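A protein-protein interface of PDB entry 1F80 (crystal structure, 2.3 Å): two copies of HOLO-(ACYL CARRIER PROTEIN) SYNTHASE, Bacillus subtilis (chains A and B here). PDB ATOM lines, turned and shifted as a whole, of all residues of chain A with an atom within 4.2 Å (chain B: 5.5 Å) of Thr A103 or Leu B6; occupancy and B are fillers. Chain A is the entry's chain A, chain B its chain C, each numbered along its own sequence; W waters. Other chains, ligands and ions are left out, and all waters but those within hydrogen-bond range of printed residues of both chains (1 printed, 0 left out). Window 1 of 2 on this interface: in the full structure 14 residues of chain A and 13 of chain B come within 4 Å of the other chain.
The backbone carbonyl oxygen (O) of Gln A112 sits at hydrogen-bond distance from the backbone NH (N) of Ser A101 (3.1 Å).
N of Thr A103 lies within hydrogen-bond range of O of Ala A110 (2.9 Å).
O of Gly B5 sits at hydrogen-bond distance from N of Val B113 (2.8 Å).
The side-chain amino group (NZ) of Lys B61 lies within hydrogen-bond range of the backbone carbonyl oxygen (O) of Leu B6, at 3.4 Å.
The backbone carbonyl oxygen (O) of Asp B7 sits at hydrogen-bond distance from the backbone NH (N) of Ala B111 (2.9 Å).
Gln A112 touches its own counterpart, Gln B112.
Position printed for both chains: 112.
Among the printed residues, merely in contact across the chains: Ser A101 with Ile B4 (3.6 Å), Ser A101 with Gly B5 (3.5 Å), Ser A101 with Lys B61 (3.7 Å), Thr A103 with Leu B6 (3.5 Å), Thr A103 with Ile B8 (3.7 Å), Thr A103 with Lys B61 (3.5 Å), Ala A110 with Ile B8 (3.7 Å), Gln A112 with Ile B4 (3.7 Å) and Gln A112 with Leu B6 (3.5 Å).
OG of Ser A101 is in hydrogen-bond range of N of Leu B6.
OG1 of Thr A103 is in hydrogen-bond range of OD2 of Asp B7 (3.3 Å).
NE2 of Gln A112 sits at hydrogen-bond distance from O of Gly B5, 3.2 Å away.
OE1 of Gln A112 lies close to OE1 of Gln B112 (3.3 Å).
The backbone carbonyl oxygen (O) of Ile A102 lies close to the side-chain amino group (NZ) of Lys B61, at 2.3 Å.
Water W1 lies within hydrogen-bond range of the side-chain amide nitrogen of Gln A112 (2.6 Å), the backbone carbonyl oxygen of Val B113 (3.1 Å) and the side-chain amide oxygen of Gln B112 (3.2 Å).
Of the 10 printed residues of chain B, 7 touch a printed residue of chain A.
Hydrophobic or aromatic side chains of chain B that line the printed part of chain A: Ile B4, Leu B6 and Ile B8.
Of the 8 printed residues of chain A, 5 touch a printed residue of chain B.
Hydrophobic or aromatic side chains of chain A within 4 Å of the printed part of chain B: Ala A110.
Printed residues of chain B within 4 Å of Ile A102: Lys B61.
Of the printed residues of chain B, Thr A103 touches Leu B6 (3.5 Å), Asp B7 (3.3 Å), Ile B8 (3.7 Å) and Lys B61 (3.5 Å).
Printed residues of chain A within 4 Å of Gly B5: Ser A101 (3.5 Å) and Gln A112 (3.2 Å).
Leu B6 touches three residues of chain A.
Of the printed residues of chain A, Lys B61 touches Ser A101, Ile A102 and Thr A103.
The nearest printed residue of chain A that does not touch Leu B6 is Ala A110 (4.2 Å).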
ATOM      1  N   SER A 101      -3.376  12.077 -15.032  1.00  0.00           N
ATOM      2  CA  SER A 101      -2.162  11.377 -15.422  1.00  0.00           C
ATOM      3  C   SER A 101      -2.051  11.301 -16.942  1.00  0.00           C
ATOM      4  O   SER A 101      -2.994  10.969 -17.648  1.00  0.00           O
ATOM      5  CB  SER A 101      -2.205   9.966 -14.828  1.00  0.00           C
ATOM      6  OG  SER A 101      -0.959   9.311 -15.057  1.00  0.00           O
ATOM      7  N   ILE A 102      -0.866  11.671 -17.446  1.00  0.00           N
ATOM      8  CA  ILE A 102      -0.679  11.667 -18.890  1.00  0.00           C
ATOM      9  C   ILE A 102       0.448  10.725 -19.309  1.00  0.00           C
ATOM     10  O   ILE A 102       1.487  10.615 -18.674  1.00  0.00           O
ATOM     11  CB  ILE A 102      -0.359  13.094 -19.330  1.00  0.00           C
ATOM     12  CG1 ILE A 102      -1.491  14.039 -18.927  1.00  0.00           C
ATOM     13  CG2 ILE A 102      -0.218  13.149 -20.862  1.00  0.00           C
ATOM     14  CD1 ILE A 102      -1.036  15.499 -18.880  1.00  0.00           C
ATOM     15  N   THR A 103       0.188   9.989 -20.401  1.00  0.00           N
ATOM     16  CA  THR A 103       1.214   9.093 -20.913  1.00  0.00           C
ATOM     17  C   THR A 103       1.262   9.111 -22.438  1.00  0.00           C
ATOM     18  O   THR A 103       0.306   9.470 -23.113  1.00  0.00           O
ATOM     19  CB  THR A 103       0.909   7.681 -20.424  1.00  0.00           C
ATOM     20  OG1 THR A 103       2.077   6.875 -20.576  1.00  0.00           O
ATOM     21  CG2 THR A 103      -0.219   7.073 -21.264  1.00  0.00           C
ATOM     22  N   HIS A 104       2.387   8.717 -23.007  1.00  0.00           N
ATOM     23  CA  HIS A 104       2.617   8.810 -24.440  1.00  0.00           C
ATOM     24  C   HIS A 104       3.202   7.517 -25.020  1.00  0.00           C
ATOM     25  O   HIS A 104       4.084   6.887 -24.446  1.00  0.00           O
ATOM     26  CB  HIS A 104       3.626   9.934 -24.668  1.00  0.00           C
ATOM     27  CG  HIS A 104       2.965  11.267 -24.462  1.00  0.00           C
ATOM     28  ND1 HIS A 104       2.327  11.936 -25.456  1.00  0.00           N
ATOM     29  CD2 HIS A 104       3.018  12.090 -23.334  1.00  0.00           C
ATOM     30  CE1 HIS A 104       2.004  13.138 -24.938  1.00  0.00           C
ATOM     31  NE2 HIS A 104       2.406  13.256 -23.669  1.00  0.00           N
ATOM     32  N   TYR A 108       0.412   7.527 -29.747  1.00  0.00           N
ATOM     33  CA  TYR A 108      -0.672   8.090 -28.931  1.00  0.00           C
ATOM     34  C   TYR A 108      -0.361   8.953 -27.732  1.00  0.00           C
ATOM     35  O   TYR A 108       0.692   8.819 -27.098  1.00  0.00           O
ATOM     36  CB  TYR A 108      -1.549   6.960 -28.364  1.00  0.00           C
ATOM     37  CG  TYR A 108      -2.144   6.029 -29.374  1.00  0.00           C
ATOM     38  CD1 TYR A 108      -3.162   6.441 -30.212  1.00  0.00           C
ATOM     39  CD2 TYR A 108      -1.655   4.741 -29.508  1.00  0.00           C
ATOM     40  CE1 TYR A 108      -3.678   5.599 -31.159  1.00  0.00           C
ATOM     41  CE2 TYR A 108      -2.149   3.889 -30.458  1.00  0.00           C
ATOM     42  CZ  TYR A 108      -3.162   4.327 -31.287  1.00  0.00           C
ATOM     43  OH  TYR A 108      -3.590   3.503 -32.287  1.00  0.00           O
ATOM     44  N   ALA A 109      -1.344   9.792 -27.412  1.00  0.00           N
ATOM     45  CA  ALA A 109      -1.366  10.601 -26.179  1.00  0.00           C
ATOM     46  C   ALA A 109      -2.625  10.052 -25.432  1.00  0.00           C
ATOM     47  O   ALA A 109      -3.724   9.924 -26.016  1.00  0.00           O
ATOM     48  CB  ALA A 109      -1.555  12.041 -26.486  1.00  0.00           C
ATOM     49  N   ALA A 110      -2.469   9.658 -24.177  1.00  0.00           N
ATOM     50  CA  ALA A 110      -3.608   9.193 -23.406  1.00  0.00           C
ATOM     51  C   ALA A 110      -3.593   9.930 -22.060  1.00  0.00           C
ATOM     52  O   ALA A 110      -2.519  10.188 -21.506  1.00  0.00           O
ATOM     53  CB  ALA A 110      -3.500   7.756 -23.157  1.00  0.00           C
ATOM     54  N   GLN A 112      -6.043  10.354 -18.155  1.00  0.00           N
ATOM     55  CA  GLN A 112      -7.165   9.947 -17.356  1.00  0.00           C
ATOM     56  C   GLN A 112      -7.298  11.039 -16.278  1.00  0.00           C
ATOM     57  O   GLN A 112      -6.297  11.652 -15.835  1.00  0.00           O
ATOM     58  CB  GLN A 112      -6.956   8.551 -16.754  1.00  0.00           C
ATOM     59  CG  GLN A 112      -6.071   8.474 -15.626  1.00  0.00           C
ATOM     60  CD  GLN A 112      -5.859   7.031 -15.223  1.00  0.00           C
ATOM     61  OE1 GLN A 112      -6.477   6.124 -15.800  1.00  0.00           O
ATOM     62  NE2 GLN A 112      -4.978   6.799 -14.261  1.00  0.00           N
ATOM     63  N   ILE B   4      -3.232   9.390  -9.104  1.00  0.00           N
ATOM     64  CA  ILE B   4      -3.511   8.294  -9.982  1.00  0.00           C
ATOM     65  C   ILE B   4      -2.394   8.242 -11.021  1.00  0.00           C
ATOM     66  O   ILE B   4      -1.747   9.251 -11.320  1.00  0.00           O
ATOM     67  CB  ILE B   4      -4.873   8.457 -10.674  1.00  0.00           C
ATOM     68  CG1 ILE B   4      -4.814   9.631 -11.685  1.00  0.00           C
ATOM     69  CG2 ILE B   4      -5.947   8.639  -9.637  1.00  0.00           C
ATOM     70  CD1 ILE B   4      -6.174  10.031 -12.249  1.00  0.00           C
ATOM     71  N   GLY B   5      -2.152   7.046 -11.545  1.00  0.00           N
ATOM     72  CA  GLY B   5      -1.136   6.883 -12.568  1.00  0.00           C
ATOM     73  C   GLY B   5      -1.649   6.005 -13.706  1.00  0.00           C
ATOM     74  O   GLY B   5      -2.386   5.036 -13.518  1.00  0.00           O
ATOM     75  N   LEU B   6      -1.251   6.365 -14.904  1.00  0.00           N
ATOM     76  CA  LEU B   6      -1.628   5.639 -16.085  1.00  0.00           C
ATOM     77  C   LEU B   6      -0.416   5.451 -16.973  1.00  0.00           C
ATOM     78  O   LEU B   6       0.315   6.414 -17.222  1.00  0.00           O
ATOM     79  CB  LEU B   6      -2.658   6.441 -16.897  1.00  0.00           C
ATOM     80  CG  LEU B   6      -2.879   5.809 -18.290  1.00  0.00           C
ATOM     81  CD1 LEU B   6      -3.404   4.383 -18.059  1.00  0.00           C
ATOM     82  CD2 LEU B   6      -3.836   6.630 -19.152  1.00  0.00           C
ATOM     83  N   ASP B   7      -0.181   4.239 -17.454  1.00  0.00           N
ATOM     84  CA  ASP B   7       0.911   4.066 -18.412  1.00  0.00           C
ATOM     85  C   ASP B   7       0.551   3.066 -19.497  1.00  0.00           C
ATOM     86  O   ASP B   7      -0.125   2.088 -19.221  1.00  0.00           O
ATOM     87  CB  ASP B   7       2.230   3.629 -17.771  1.00  0.00           C
ATOM     88  CG  ASP B   7       3.343   3.445 -18.840  1.00  0.00           C
ATOM     89  OD1 ASP B   7       3.616   2.282 -19.238  1.00  0.00           O
ATOM     90  OD2 ASP B   7       3.923   4.472 -19.324  1.00  0.00           O
ATOM     91  N   ILE B   8       0.995   3.331 -20.720  1.00  0.00           N
ATOM     92  CA  ILE B   8       0.774   2.460 -21.858  1.00  0.00           C
ATOM     93  C   ILE B   8       2.152   2.210 -22.532  1.00  0.00           C
ATOM     94  O   ILE B   8       2.751   3.142 -23.076  1.00  0.00           O
ATOM     95  CB  ILE B   8      -0.178   3.097 -22.901  1.00  0.00           C
ATOM     96  CG1 ILE B   8      -1.545   3.421 -22.294  1.00  0.00           C
ATOM     97  CG2 ILE B   8      -0.399   2.116 -24.043  1.00  0.00           C
ATOM     98  CD1 ILE B   8      -2.438   4.263 -23.240  1.00  0.00           C
ATOM     99  N   ALA B  58       3.020   3.339 -13.725  1.00  0.00           N
ATOM    100  CA  ALA B  58       1.738   3.928 -13.348  1.00  0.00           C
ATOM    101  C   ALA B  58       1.779   4.216 -11.867  1.00  0.00           C
ATOM    102  O   ALA B  58       1.348   5.254 -11.412  1.00  0.00           O
ATOM    103  CB  ALA B  58       0.588   2.983 -13.629  1.00  0.00           C
ATOM    104  N   LYS B  61       3.873   7.178 -11.179  1.00  0.00           N
ATOM    105  CA  LYS B  61       3.278   8.468 -11.507  1.00  0.00           C
ATOM    106  C   LYS B  61       2.304   8.816 -10.412  1.00  0.00           C
ATOM    107  O   LYS B  61       2.339   9.931  -9.919  1.00  0.00           O
ATOM    108  CB  LYS B  61       2.578   8.440 -12.834  1.00  0.00           C
ATOM    109  CG  LYS B  61       3.513   8.323 -14.024  1.00  0.00           C
ATOM    110  CD  LYS B  61       2.641   8.316 -15.254  1.00  0.00           C
ATOM    111  CE  LYS B  61       3.427   8.236 -16.510  1.00  0.00           C
ATOM    112  NZ  LYS B  61       2.620   8.896 -17.575  1.00  0.00           N
ATOM    113  N   ALA B 111      -1.540  -0.028 -17.848  1.00  0.00           N
ATOM    114  CA  ALA B 111      -1.850  -0.217 -16.426  1.00  0.00           C
ATOM    115  C   ALA B 111      -2.302   1.079 -15.788  1.00  0.00           C
ATOM    116  O   ALA B 111      -1.962   2.166 -16.224  1.00  0.00           O
ATOM    117  CB  ALA B 111      -0.634  -0.756 -15.671  1.00  0.00           C
ATOM    118  N   GLN B 112      -3.085   0.964 -14.747  1.00  0.00           N
ATOM    119  CA  GLN B 112      -3.509   2.169 -14.078  1.00  0.00           C
ATOM    120  C   GLN B 112      -3.403   1.900 -12.612  1.00  0.00           C
ATOM    121  O   GLN B 112      -3.522   0.768 -12.154  1.00  0.00           O
ATOM    122  CB  GLN B 112      -4.945   2.554 -14.447  1.00  0.00           C
ATOM    123  CG  GLN B 112      -6.010   1.563 -14.071  1.00  0.00           C
ATOM    124  CD  GLN B 112      -7.427   2.130 -14.337  1.00  0.00           C
ATOM    125  OE1 GLN B 112      -7.609   3.336 -14.391  1.00  0.00           O
ATOM    126  NE2 GLN B 112      -8.402   1.270 -14.484  1.00  0.00           N
ATOM    127  N   VAL B 113      -3.154   2.960 -11.877  1.00  0.00           N
ATOM    128  CA  VAL B 113      -3.026   2.828 -10.453  1.00  0.00           C
ATOM    129  C   VAL B 113      -3.724   3.999  -9.768  1.00  0.00           C
ATOM    130  O   VAL B 113      -3.724   5.102 -10.269  1.00  0.00           O
ATOM    131  CB  VAL B 113      -1.506   2.848 -10.022  1.00  0.00           C
ATOM    132  CG1 VAL B 113      -1.398   3.175  -8.501  1.00  0.00           C
ATOM    133  CG2 VAL B 113      -0.848   1.487 -10.310  1.00  0.00           C
HETATM  134  O   HOH W   1      -6.009   5.253 -12.429  1.00  0.00           O
